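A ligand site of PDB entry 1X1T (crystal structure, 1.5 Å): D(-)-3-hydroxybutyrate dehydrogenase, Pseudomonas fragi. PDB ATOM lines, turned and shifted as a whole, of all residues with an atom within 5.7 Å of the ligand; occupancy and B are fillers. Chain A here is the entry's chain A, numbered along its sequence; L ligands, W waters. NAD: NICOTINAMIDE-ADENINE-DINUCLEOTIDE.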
ATOM      1  N   THR A  10     -20.695 -16.542 -20.431  1.00  0.00           N
ATOM      2  CA  THR A  10     -21.857 -15.673 -20.301  1.00  0.00           C
ATOM      3  C   THR A  10     -21.612 -14.667 -19.189  1.00  0.00           C
ATOM      4  O   THR A  10     -20.908 -14.948 -18.224  1.00  0.00           O
ATOM      5  CB  THR A  10     -23.152 -16.469 -19.993  1.00  0.00           C
ATOM      6  OG1 THR A  10     -23.083 -17.016 -18.670  1.00  0.00           O
ATOM      7  CG2 THR A  10     -23.329 -17.596 -21.007  1.00  0.00           C
ATOM      8  N   GLY A  11     -22.178 -13.468 -19.344  1.00  0.00           N
ATOM      9  CA  GLY A  11     -21.990 -12.437 -18.334  1.00  0.00           C
ATOM     10  C   GLY A  11     -20.522 -12.129 -18.102  1.00  0.00           C
ATOM     11  O   GLY A  11     -20.073 -12.043 -16.964  1.00  0.00           O
ATOM     12  N   SER A  12     -19.786 -11.935 -19.194  1.00  0.00           N
ATOM     13  CA  SER A  12     -18.358 -11.651 -19.119  1.00  0.00           C
ATOM     14  C   SER A  12     -17.985 -10.211 -19.443  1.00  0.00           C
ATOM     15  O   SER A  12     -16.829  -9.919 -19.734  1.00  0.00           O
ATOM     16  CB  SER A  12     -17.585 -12.605 -20.039  1.00  0.00           C
ATOM     17  OG  SER A  12     -18.195 -12.704 -21.314  1.00  0.00           O
ATOM     18  N   THR A  13     -18.964  -9.311 -19.383  1.00  0.00           N
ATOM     19  CA  THR A  13     -18.682  -7.908 -19.657  1.00  0.00           C
ATOM     20  C   THR A  13     -18.157  -7.216 -18.407  1.00  0.00           C
ATOM     21  O   THR A  13     -17.734  -6.058 -18.461  1.00  0.00           O
ATOM     22  CB  THR A  13     -19.953  -7.173 -20.155  1.00  0.00           C
ATOM     23  OG1 THR A  13     -21.052  -7.423 -19.268  1.00  0.00           O
ATOM     24  CG2 THR A  13     -20.315  -7.626 -21.569  1.00  0.00           C
ATOM     25  N   SER A  14     -18.159  -7.932 -17.288  1.00  0.00           N
ATOM     26  CA  SER A  14     -17.659  -7.389 -16.029  1.00  0.00           C
ATOM     27  C   SER A  14     -17.545  -8.465 -14.949  1.00  0.00           C
ATOM     28  O   SER A  14     -17.895  -9.626 -15.187  1.00  0.00           O
ATOM     29  CB  SER A  14     -18.600  -6.285 -15.523  1.00  0.00           C
ATOM     30  OG  SER A  14     -19.876  -6.804 -15.217  1.00  0.00           O
ATOM     31  N   GLY A  15     -17.045  -8.064 -13.784  1.00  0.00           N
ATOM     32  CA  GLY A  15     -16.904  -8.958 -12.656  1.00  0.00           C
ATOM     33  C   GLY A  15     -16.207 -10.300 -12.880  1.00  0.00           C
ATOM     34  O   GLY A  15     -15.197 -10.397 -13.581  1.00  0.00           O
ATOM     35  N   ILE A  16     -16.776 -11.319 -12.256  1.00  0.00           N
ATOM     36  CA  ILE A  16     -16.251 -12.683 -12.334  1.00  0.00           C
ATOM     37  C   ILE A  16     -16.137 -13.209 -13.760  1.00  0.00           C
ATOM     38  O   ILE A  16     -15.116 -13.788 -14.141  1.00  0.00           O
ATOM     39  CB  ILE A  16     -17.133 -13.643 -11.501  1.00  0.00           C
ATOM     40  CG1 ILE A  16     -17.056 -13.233 -10.020  1.00  0.00           C
ATOM     41  CG2 ILE A  16     -16.670 -15.085 -11.689  1.00  0.00           C
ATOM     42  CD1 ILE A  16     -18.053 -13.948  -9.140  1.00  0.00           C
ATOM     43  N   GLY A  17     -17.182 -12.998 -14.555  1.00  0.00           N
ATOM     44  CA  GLY A  17     -17.184 -13.463 -15.929  1.00  0.00           C
ATOM     45  C   GLY A  17     -16.041 -12.883 -16.737  1.00  0.00           C
ATOM     46  O   GLY A  17     -15.393 -13.593 -17.518  1.00  0.00           O
ATOM     47  N   ASN A  34     -20.096 -11.941 -23.560  1.00  0.00           N
ATOM     48  CA  ASN A  34     -21.542 -11.752 -23.529  1.00  0.00           C
ATOM     49  C   ASN A  34     -21.943 -10.994 -22.280  1.00  0.00           C
ATOM     50  O   ASN A  34     -21.232 -11.017 -21.269  1.00  0.00           O
ATOM     51  CB  ASN A  34     -22.238 -13.130 -23.557  1.00  0.00           C
ATOM     52  CG  ASN A  34     -23.654 -13.084 -23.029  1.00  0.00           C
ATOM     53  OD1 ASN A  34     -23.896 -13.284 -21.834  1.00  0.00           O
ATOM     54  ND2 ASN A  34     -24.610 -12.807 -23.915  1.00  0.00           N
ATOM     55  N   GLY A  35     -23.079 -10.314 -22.339  1.00  0.00           N
ATOM     56  CA  GLY A  35     -23.550  -9.567 -21.190  1.00  0.00           C
ATOM     57  C   GLY A  35     -24.021  -8.166 -21.533  1.00  0.00           C
ATOM     58  O   GLY A  35     -23.857  -7.704 -22.656  1.00  0.00           O
ATOM     59  N   PHE A  36     -24.611  -7.517 -20.546  1.00  0.00           N
ATOM     60  CA  PHE A  36     -25.122  -6.156 -20.716  1.00  0.00           C
ATOM     61  C   PHE A  36     -24.031  -5.159 -20.394  1.00  0.00           C
ATOM     62  O   PHE A  36     -22.994  -5.507 -19.827  1.00  0.00           O
ATOM     63  CB  PHE A  36     -26.323  -5.933 -19.800  1.00  0.00           C
ATOM     64  CG  PHE A  36     -27.520  -6.762 -20.159  1.00  0.00           C
ATOM     65  CD1 PHE A  36     -28.521  -7.006 -19.223  1.00  0.00           C
ATOM     66  CD2 PHE A  36     -27.667  -7.286 -21.443  1.00  0.00           C
ATOM     67  CE1 PHE A  36     -29.644  -7.748 -19.560  1.00  0.00           C
ATOM     68  CE2 PHE A  36     -28.792  -8.037 -21.785  1.00  0.00           C
ATOM     69  CZ  PHE A  36     -29.784  -8.270 -20.849  1.00  0.00           C
ATOM     70  N   GLY A  37     -24.263  -3.903 -20.754  1.00  0.00           N
ATOM     71  CA  GLY A  37     -23.275  -2.883 -20.488  1.00  0.00           C
ATOM     72  C   GLY A  37     -23.163  -1.897 -21.627  1.00  0.00           C
ATOM     73  O   GLY A  37     -23.913  -1.951 -22.608  1.00  0.00           O
ATOM     74  N   ALA A  62     -26.563 -11.203 -26.325  1.00  0.00           N
ATOM     75  CA  ALA A  62     -27.803 -11.935 -26.122  1.00  0.00           C
ATOM     76  C   ALA A  62     -28.340 -11.798 -24.704  1.00  0.00           C
ATOM     77  O   ALA A  62     -27.593 -11.892 -23.737  1.00  0.00           O
ATOM     78  CB  ALA A  62     -27.596 -13.415 -26.450  1.00  0.00           C
ATOM     79  N   ASP A  63     -29.649 -11.562 -24.582  1.00  0.00           N
ATOM     80  CA  ASP A  63     -30.318 -11.434 -23.295  1.00  0.00           C
ATOM     81  C   ASP A  63     -30.629 -12.858 -22.859  1.00  0.00           C
ATOM     82  O   ASP A  63     -31.577 -13.477 -23.332  1.00  0.00           O
ATOM     83  CB  ASP A  63     -31.599 -10.619 -23.443  1.00  0.00           C
ATOM     84  CG  ASP A  63     -32.360 -10.475 -22.130  1.00  0.00           C
ATOM     85  OD1 ASP A  63     -33.296  -9.643 -22.083  1.00  0.00           O
ATOM     86  OD2 ASP A  63     -32.034 -11.180 -21.164  1.00  0.00           O
ATOM     87  N   LEU A  64     -29.830 -13.370 -21.925  1.00  0.00           N
ATOM     88  CA  LEU A  64     -29.987 -14.742 -21.463  1.00  0.00           C
ATOM     89  C   LEU A  64     -31.227 -15.055 -20.625  1.00  0.00           C
ATOM     90  O   LEU A  64     -31.369 -16.173 -20.129  1.00  0.00           O
ATOM     91  CB  LEU A  64     -28.716 -15.175 -20.730  1.00  0.00           C
ATOM     92  CG  LEU A  64     -27.458 -14.964 -21.582  1.00  0.00           C
ATOM     93  CD1 LEU A  64     -26.242 -15.489 -20.831  1.00  0.00           C
ATOM     94  CD2 LEU A  64     -27.603 -15.667 -22.925  1.00  0.00           C
ATOM     95  N   SER A  65     -32.115 -14.081 -20.454  1.00  0.00           N
ATOM     96  CA  SER A  65     -33.338 -14.320 -19.692  1.00  0.00           C
ATOM     97  C   SER A  65     -34.325 -15.044 -20.615  1.00  0.00           C
ATOM     98  O   SER A  65     -35.374 -15.529 -20.176  1.00  0.00           O
ATOM     99  CB  SER A  65     -33.945 -12.998 -19.217  1.00  0.00           C
ATOM    100  OG  SER A  65     -34.401 -12.214 -20.299  1.00  0.00           O
ATOM    101  N   ASN A  90     -22.108 -18.208 -16.445  1.00  0.00           N
ATOM    102  CA  ASN A  90     -21.825 -17.301 -15.336  1.00  0.00           C
ATOM    103  C   ASN A  90     -22.845 -16.201 -15.028  1.00  0.00           C
ATOM    104  O   ASN A  90     -23.005 -15.837 -13.859  1.00  0.00           O
ATOM    105  CB  ASN A  90     -20.453 -16.677 -15.595  1.00  0.00           C
ATOM    106  CG  ASN A  90     -20.140 -15.519 -14.683  1.00  0.00           C
ATOM    107  OD1 ASN A  90     -19.744 -15.702 -13.533  1.00  0.00           O
ATOM    108  ND2 ASN A  90     -20.329 -14.304 -15.185  1.00  0.00           N
ATOM    109  N   ALA A  91     -23.525 -15.673 -16.040  1.00  0.00           N
ATOM    110  CA  ALA A  91     -24.496 -14.601 -15.805  1.00  0.00           C
ATOM    111  C   ALA A  91     -25.467 -14.893 -14.659  1.00  0.00           C
ATOM    112  O   ALA A  91     -25.987 -15.996 -14.528  1.00  0.00           O
ATOM    113  CB  ALA A  91     -25.275 -14.318 -17.085  1.00  0.00           C
ATOM    114  N   GLY A  92     -25.711 -13.885 -13.823  1.00  0.00           N
ATOM    115  CA  GLY A  92     -26.618 -14.066 -12.707  1.00  0.00           C
ATOM    116  C   GLY A  92     -27.043 -12.774 -12.051  1.00  0.00           C
ATOM    117  O   GLY A  92     -26.356 -11.760 -12.163  1.00  0.00           O
ATOM    118  N   ILE A  93     -28.181 -12.810 -11.368  1.00  0.00           N
ATOM    119  CA  ILE A  93     -28.723 -11.642 -10.655  1.00  0.00           C
ATOM    120  C   ILE A  93     -29.175 -12.056  -9.258  1.00  0.00           C
ATOM    121  O   ILE A  93     -29.240 -13.241  -8.944  1.00  0.00           O
ATOM    122  CB  ILE A  93     -29.928 -11.028 -11.414  1.00  0.00           C
ATOM    123  CG1 ILE A  93     -30.973 -12.112 -11.686  1.00  0.00           C
ATOM    124  CG2 ILE A  93     -29.459 -10.380 -12.712  1.00  0.00           C
ATOM    125  CD1 ILE A  93     -32.274 -11.584 -12.249  1.00  0.00           C
ATOM    126  N   LEU A 113     -32.663 -16.625 -15.232  1.00  0.00           N
ATOM    127  CA  LEU A 113     -31.275 -16.367 -15.561  1.00  0.00           C
ATOM    128  C   LEU A 113     -30.278 -17.249 -14.824  1.00  0.00           C
ATOM    129  O   LEU A 113     -29.394 -17.842 -15.434  1.00  0.00           O
ATOM    130  CB  LEU A 113     -30.918 -14.902 -15.292  1.00  0.00           C
ATOM    131  CG  LEU A 113     -29.479 -14.514 -15.641  1.00  0.00           C
ATOM    132  CD1 LEU A 113     -29.228 -14.684 -17.131  1.00  0.00           C
ATOM    133  CD2 LEU A 113     -29.223 -13.078 -15.223  1.00  0.00           C
ATOM    134  N   ASN A 114     -30.419 -17.339 -13.503  1.00  0.00           N
ATOM    135  CA  ASN A 114     -29.505 -18.114 -12.679  1.00  0.00           C
ATOM    136  C   ASN A 114     -29.599 -19.624 -12.847  1.00  0.00           C
ATOM    137  O   ASN A 114     -28.630 -20.330 -12.584  1.00  0.00           O
ATOM    138  CB  ASN A 114     -29.696 -17.742 -11.210  1.00  0.00           C
ATOM    139  CG  ASN A 114     -29.343 -16.301 -10.923  1.00  0.00           C
ATOM    140  OD1 ASN A 114     -29.461 -15.440 -11.789  1.00  0.00           O
ATOM    141  ND2 ASN A 114     -28.930 -16.019  -9.693  1.00  0.00           N
ATOM    142  N   ILE A 140     -20.966 -21.327 -12.872  1.00  0.00           N
ATOM    143  CA  ILE A 140     -20.631 -20.520 -11.712  1.00  0.00           C
ATOM    144  C   ILE A 140     -21.847 -20.480 -10.808  1.00  0.00           C
ATOM    145  O   ILE A 140     -22.798 -19.735 -11.043  1.00  0.00           O
ATOM    146  CB  ILE A 140     -20.207 -19.091 -12.098  1.00  0.00           C
ATOM    147  CG1 ILE A 140     -19.088 -19.139 -13.138  1.00  0.00           C
ATOM    148  CG2 ILE A 140     -19.753 -18.329 -10.852  1.00  0.00           C
ATOM    149  CD1 ILE A 140     -17.876 -19.972 -12.719  1.00  0.00           C
ATOM    150  N   ALA A 141     -21.810 -21.322  -9.778  1.00  0.00           N
ATOM    151  CA  ALA A 141     -22.905 -21.390  -8.821  1.00  0.00           C
ATOM    152  C   ALA A 141     -22.612 -20.402  -7.707  1.00  0.00           C
ATOM    153  O   ALA A 141     -22.539 -19.196  -7.947  1.00  0.00           O
ATOM    154  CB  ALA A 141     -23.034 -22.809  -8.276  1.00  0.00           C
ATOM    155  N   SER A 142     -22.413 -20.906  -6.485  1.00  0.00           N
ATOM    156  CA  SER A 142     -22.146 -20.066  -5.328  1.00  0.00           C
ATOM    157  C   SER A 142     -22.057 -20.954  -4.092  1.00  0.00           C
ATOM    158  O   SER A 142     -22.408 -22.131  -4.144  1.00  0.00           O
ATOM    159  CB  SER A 142     -23.296 -19.073  -5.131  1.00  0.00           C
ATOM    160  OG  SER A 142     -23.211 -18.414  -3.876  1.00  0.00           O
ATOM    161  N   ALA A 143     -21.587 -20.399  -2.990  1.00  0.00           N
ATOM    162  CA  ALA A 143     -21.569 -21.156  -1.743  1.00  0.00           C
ATOM    163  C   ALA A 143     -23.055 -21.420  -1.480  1.00  0.00           C
ATOM    164  O   ALA A 143     -23.420 -22.397  -0.839  1.00  0.00           O
ATOM    165  CB  ALA A 143     -20.979 -20.301  -0.617  1.00  0.00           C
ATOM    166  N   TYR A 155     -32.377 -16.974  -5.038  1.00  0.00           N
ATOM    167  CA  TYR A 155     -30.970 -17.170  -5.394  1.00  0.00           C
ATOM    168  C   TYR A 155     -30.441 -18.526  -4.929  1.00  0.00           C
ATOM    169  O   TYR A 155     -29.802 -19.246  -5.693  1.00  0.00           O
ATOM    170  CB  TYR A 155     -30.143 -16.029  -4.800  1.00  0.00           C
ATOM    171  CG  TYR A 155     -28.699 -15.989  -5.226  1.00  0.00           C
ATOM    172  CD1 TYR A 155     -27.713 -16.589  -4.457  1.00  0.00           C
ATOM    173  CD2 TYR A 155     -28.323 -15.306  -6.384  1.00  0.00           C
ATOM    174  CE1 TYR A 155     -26.372 -16.498  -4.817  1.00  0.00           C
ATOM    175  CE2 TYR A 155     -26.989 -15.211  -6.751  1.00  0.00           C
ATOM    176  CZ  TYR A 155     -26.017 -15.808  -5.965  1.00  0.00           C
ATOM    177  OH  TYR A 155     -24.694 -15.687  -6.315  1.00  0.00           O
ATOM    178  N   LYS A 159     -29.290 -21.527  -7.334  1.00  0.00           N
ATOM    179  CA  LYS A 159     -27.926 -22.025  -7.273  1.00  0.00           C
ATOM    180  C   LYS A 159     -27.850 -23.501  -6.888  1.00  0.00           C
ATOM    181  O   LYS A 159     -26.993 -24.233  -7.396  1.00  0.00           O
ATOM    182  CB  LYS A 159     -27.096 -21.174  -6.301  1.00  0.00           C
ATOM    183  CG  LYS A 159     -26.874 -19.737  -6.798  1.00  0.00           C
ATOM    184  CD  LYS A 159     -26.098 -19.697  -8.116  1.00  0.00           C
ATOM    185  CE  LYS A 159     -25.724 -18.267  -8.498  1.00  0.00           C
ATOM    186  NZ  LYS A 159     -24.940 -18.207  -9.776  1.00  0.00           N
ATOM    187  N   CYS A 184     -18.157 -22.809  -6.903  1.00  0.00           N
ATOM    188  CA  CYS A 184     -19.016 -22.196  -5.895  1.00  0.00           C
ATOM    189  C   CYS A 184     -18.269 -21.134  -5.099  1.00  0.00           C
ATOM    190  O   CYS A 184     -17.683 -21.425  -4.051  1.00  0.00           O
ATOM    191  CB  CYS A 184     -19.555 -23.297  -4.973  1.00  0.00           C
ATOM    192  SG  CYS A 184     -20.624 -24.507  -5.826  1.00  0.00           S
ATOM    193  N   PRO A 185     -18.290 -19.885  -5.586  1.00  0.00           N
ATOM    194  CA  PRO A 185     -17.589 -18.816  -4.885  1.00  0.00           C
ATOM    195  C   PRO A 185     -18.257 -18.266  -3.632  1.00  0.00           C
ATOM    196  O   PRO A 185     -19.474 -18.327  -3.476  1.00  0.00           O
ATOM    197  CB  PRO A 185     -17.465 -17.706  -5.941  1.00  0.00           C
ATOM    198  CG  PRO A 185     -17.772 -18.385  -7.260  1.00  0.00           C
ATOM    199  CD  PRO A 185     -18.817 -19.402  -6.876  1.00  0.00           C
ATOM    200  N   GLY A 186     -17.419 -17.731  -2.749  1.00  0.00           N
ATOM    201  CA  GLY A 186     -17.887 -17.074  -1.557  1.00  0.00           C
ATOM    202  C   GLY A 186     -17.914 -15.617  -1.992  1.00  0.00           C
ATOM    203  O   GLY A 186     -18.041 -15.344  -3.188  1.00  0.00           O
ATOM    204  N   TRP A 187     -17.755 -14.680  -1.072  1.00  0.00           N
ATOM    205  CA  TRP A 187     -17.789 -13.253  -1.426  1.00  0.00           C
ATOM    206  C   TRP A 187     -16.691 -12.799  -2.382  1.00  0.00           C
ATOM    207  O   TRP A 187     -15.508 -13.100  -2.193  1.00  0.00           O
ATOM    208  CB  TRP A 187     -17.693 -12.382  -0.165  1.00  0.00           C
ATOM    209  CG  TRP A 187     -18.860 -12.475   0.767  1.00  0.00           C
ATOM    210  CD1 TRP A 187     -18.827 -12.846   2.068  1.00  0.00           C
ATOM    211  CD2 TRP A 187     -20.228 -12.134   0.474  1.00  0.00           C
ATOM    212  NE1 TRP A 187     -20.081 -12.752   2.628  1.00  0.00           N
ATOM    213  CE2 TRP A 187     -20.960 -12.322   1.665  1.00  0.00           C
ATOM    214  CE3 TRP A 187     -20.893 -11.697  -0.674  1.00  0.00           C
ATOM    215  CZ2 TRP A 187     -22.338 -12.086   1.743  1.00  0.00           C
ATOM    216  CZ3 TRP A 187     -22.271 -11.461  -0.595  1.00  0.00           C
ATOM    217  CH2 TRP A 187     -22.968 -11.649   0.608  1.00  0.00           C
ATOM    218  N   VAL A 188     -17.094 -12.036  -3.404  1.00  0.00           N
ATOM    219  CA  VAL A 188     -16.195 -11.460  -4.387  1.00  0.00           C
ATOM    220  C   VAL A 188     -16.581  -9.981  -4.447  1.00  0.00           C
ATOM    221  O   VAL A 188     -17.764  -9.653  -4.550  1.00  0.00           O
ATOM    222  CB  VAL A 188     -16.384 -12.077  -5.797  1.00  0.00           C
ATOM    223  CG1 VAL A 188     -15.450 -11.387  -6.794  1.00  0.00           C
ATOM    224  CG2 VAL A 188     -16.112 -13.560  -5.752  1.00  0.00           C
ATOM    225  N   ARG A 189     -15.588  -9.097  -4.372  1.00  0.00           N
ATOM    226  CA  ARG A 189     -15.846  -7.661  -4.386  1.00  0.00           C
ATOM    227  C   ARG A 189     -16.286  -7.128  -5.744  1.00  0.00           C
ATOM    228  O   ARG A 189     -15.555  -6.372  -6.396  1.00  0.00           O
ATOM    229  CB  ARG A 189     -14.577  -6.920  -3.924  1.00  0.00           C
ATOM    230  CG  ARG A 189     -14.765  -5.427  -3.672  1.00  0.00           C
ATOM    231  CD  ARG A 189     -15.667  -5.179  -2.475  1.00  0.00           C
ATOM    232  NE  ARG A 189     -15.779  -3.752  -2.155  1.00  0.00           N
ATOM    233  CZ  ARG A 189     -16.476  -3.269  -1.138  1.00  0.00           C
ATOM    234  NH1 ARG A 189     -17.133  -4.080  -0.326  1.00  0.00           N
ATOM    235  NH2 ARG A 189     -16.512  -1.952  -0.934  1.00  0.00           N
ATOM    236  N   THR A 190     -17.486  -7.522  -6.174  1.00  0.00           N
ATOM    237  CA  THR A 190     -18.024  -7.075  -7.462  1.00  0.00           C
ATOM    238  C   THR A 190     -19.161  -6.083  -7.247  1.00  0.00           C
ATOM    239  O   THR A 190     -19.948  -6.213  -6.314  1.00  0.00           O
ATOM    240  CB  THR A 190     -18.556  -8.254  -8.294  1.00  0.00           C
ATOM    241  OG1 THR A 190     -19.650  -8.879  -7.605  1.00  0.00           O
ATOM    242  CG2 THR A 190     -17.465  -9.282  -8.538  1.00  0.00           C
HETATM  243  PA  NAD L   1     -21.594  -8.830 -12.126  1.00  0.00           P
HETATM  244  O1A NAD L   1     -22.812  -7.982 -12.135  1.00  0.00           O
HETATM  245  O2A NAD L   1     -20.245  -8.187 -12.051  1.00  0.00           O
HETATM  246  O5B NAD L   1     -21.669  -9.770 -13.413  1.00  0.00           O
HETATM  247  C5B NAD L   1     -22.929 -10.324 -13.903  1.00  0.00           C
HETATM  248  C4B NAD L   1     -22.842 -10.380 -15.413  1.00  0.00           C
HETATM  249  O4B NAD L   1     -24.154 -10.920 -15.807  1.00  0.00           O
HETATM  250  C3B NAD L   1     -22.740  -8.986 -16.114  1.00  0.00           C
HETATM  251  O3B NAD L   1     -21.623  -9.031 -17.050  1.00  0.00           O
HETATM  252  C2B NAD L   1     -24.066  -8.776 -16.813  1.00  0.00           C
HETATM  253  O2B NAD L   1     -24.113  -7.988 -17.941  1.00  0.00           O
HETATM  254  C1B NAD L   1     -24.531 -10.230 -16.994  1.00  0.00           C
HETATM  255  N9A NAD L   1     -25.971 -10.320 -17.070  1.00  0.00           N
HETATM  256  C8A NAD L   1     -26.997 -10.007 -16.185  1.00  0.00           C
HETATM  257  N7A NAD L   1     -28.200 -10.258 -16.665  1.00  0.00           N
HETATM  258  C5A NAD L   1     -28.039 -10.757 -17.906  1.00  0.00           C
HETATM  259  C6A NAD L   1     -28.978 -11.217 -18.938  1.00  0.00           C
HETATM  260  N6A NAD L   1     -30.287 -11.209 -18.764  1.00  0.00           N
HETATM  261  N1A NAD L   1     -28.380 -11.671 -20.109  1.00  0.00           N
HETATM  262  C2A NAD L   1     -27.057 -11.699 -20.345  1.00  0.00           C
HETATM  263  N3A NAD L   1     -26.113 -11.278 -19.399  1.00  0.00           N
HETATM  264  C4A NAD L   1     -26.653 -10.805 -18.192  1.00  0.00           C
HETATM  265  O3  NAD L   1     -21.663  -9.849 -10.908  1.00  0.00           O
HETATM  266  PN  NAD L   1     -20.791 -11.160 -10.504  1.00  0.00           P
HETATM  267  O1N NAD L   1     -20.720 -11.222  -9.038  1.00  0.00           O
HETATM  268  O2N NAD L   1     -19.547 -11.176 -11.321  1.00  0.00           O
HETATM  269  O5D NAD L   1     -21.843 -12.301 -10.977  1.00  0.00           O
HETATM  270  C5D NAD L   1     -21.407 -13.382 -11.858  1.00  0.00           C
HETATM  271  C4D NAD L   1     -21.859 -14.701 -11.325  1.00  0.00           C
HETATM  272  O4D NAD L   1     -21.139 -15.002 -10.064  1.00  0.00           O
HETATM  273  C3D NAD L   1     -23.391 -14.772 -10.931  1.00  0.00           C
HETATM  274  O3D NAD L   1     -23.975 -15.998 -11.416  1.00  0.00           O
HETATM  275  C2D NAD L   1     -23.372 -14.777  -9.398  1.00  0.00           C
HETATM  276  O2D NAD L   1     -24.538 -15.332  -8.857  1.00  0.00           O
HETATM  277  C1D NAD L   1     -22.065 -15.576  -9.117  1.00  0.00           C
HETATM  278  N1N NAD L   1     -21.497 -15.444  -7.740  1.00  0.00           N
HETATM  279  C2N NAD L   1     -21.116 -14.129  -7.268  1.00  0.00           C
HETATM  280  C3N NAD L   1     -20.430 -13.973  -6.125  1.00  0.00           C
HETATM  281  C7N NAD L   1     -20.021 -12.598  -5.620  1.00  0.00           C
HETATM  282  O7N NAD L   1     -19.784 -12.477  -4.397  1.00  0.00           O
HETATM  283  N7N NAD L   1     -19.914 -11.580  -6.484  1.00  0.00           N
HETATM  284  C4N NAD L   1     -20.017 -15.177  -5.275  1.00  0.00           C
HETATM  285  C5N NAD L   1     -20.810 -16.431  -5.599  1.00  0.00           C
HETATM  286  C6N NAD L   1     -21.347 -16.585  -6.911  1.00  0.00           C
HETATM  287  O   HOH W   1     -24.008  -6.092 -13.785  1.00  0.00           O
HETATM  288  O   HOH W   2     -30.405  -8.773 -15.792  1.00  0.00           O
HETATM  289  O   HOH W   3     -19.647 -11.700 -14.031  1.00  0.00           O
HETATM  290  O   HOH W   4     -26.563  -7.599 -13.842  1.00  0.00           O
HETATM  291  O   HOH W   5     -32.453 -10.822 -16.535  1.00  0.00           O
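The side-chain amide nitrogen (ND2) of Asn 90 sits close to the backbone NH (N) of Gly 17.
N of Asn 90 sits at hydrogen-bond distance from OG1 of Thr 10, at 2.7 Å.
O of Ala 141 sits at hydrogen-bond distance from NZ of Lys 159 (3.2 Å).
O of Ile 140 lies within hydrogen-bond range of NZ of Lys 159 (2.9 Å).
OD2 of Asp 63 sits at hydrogen-bond distance from OG of Ser 65, at 2.7 Å.
O of Pro 185 is in hydrogen-bond range of N of Ala 143, 3.0 Å away.
The backbone NH of Gly 11 sits at hydrogen-bond distance from the side-chain amide oxygen of Asn 34 (3.0 Å).
O of Asn 34 lies within hydrogen-bond range of N of Ser 12 (2.7 Å).
Merely in contact with the ligand: Gly 186, Ala 141, Pro 185, Leu 113, Ala 62, Gly 15, Gly 92, Ser 142, Gly 35, Trp 187, Ile 140, Ala 91, Ser 65 and Asn 34.
An oxygen (O2D) of the ligand is in hydrogen-bond range of the side-chain hydroxyl (OH) of Tyr 155.
The backbone carbonyl oxygen (O) of Asn 90 is in hydrogen-bond range of an oxygen (O3D) of the ligand, 2.6 Å away.
The backbone NH (N) of Phe 36 is in hydrogen-bond range of an oxygen (O2B) of the ligand (2.7 Å).
O2B of the ligand is in hydrogen-bond range of O of Phe 36 (3.3 Å).
OG1 of Thr 13 sits at hydrogen-bond distance from O3B of the ligand.
N of Leu 64 is in hydrogen-bond range of N1A of the ligand, 2.9 Å away.
The backbone NH of Val 188 lies within hydrogen-bond range of an oxygen (O7N) of the ligand, at 2.9 Å.
N7N of the ligand sits at hydrogen-bond distance from O of Val 188.
The side-chain amino group (NZ) of Lys 159 sits at hydrogen-bond distance from an oxygen (O3D) of the ligand (2.9 Å).
An oxygen (O2N) of the ligand lies within hydrogen-bond range of the backbone NH (N) of Ile 16, at 2.9 Å.
OG1 of Thr 190 sits at hydrogen-bond distance from N7N of the ligand (2.9 Å).
The side-chain carboxylate (OD2) of Asp 63 lies within hydrogen-bond range of a nitrogen (N6A) of the ligand, 3.0 Å away.
The side-chain hydroxyl (OG) of Ser 14 lies within hydrogen-bond range of an oxygen (O3B) of the ligand (3.4 Å).
An oxygen (O3B) of the ligand is in hydrogen-bond range of the backbone carbonyl oxygen of Gly 11, 3.4 Å away.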
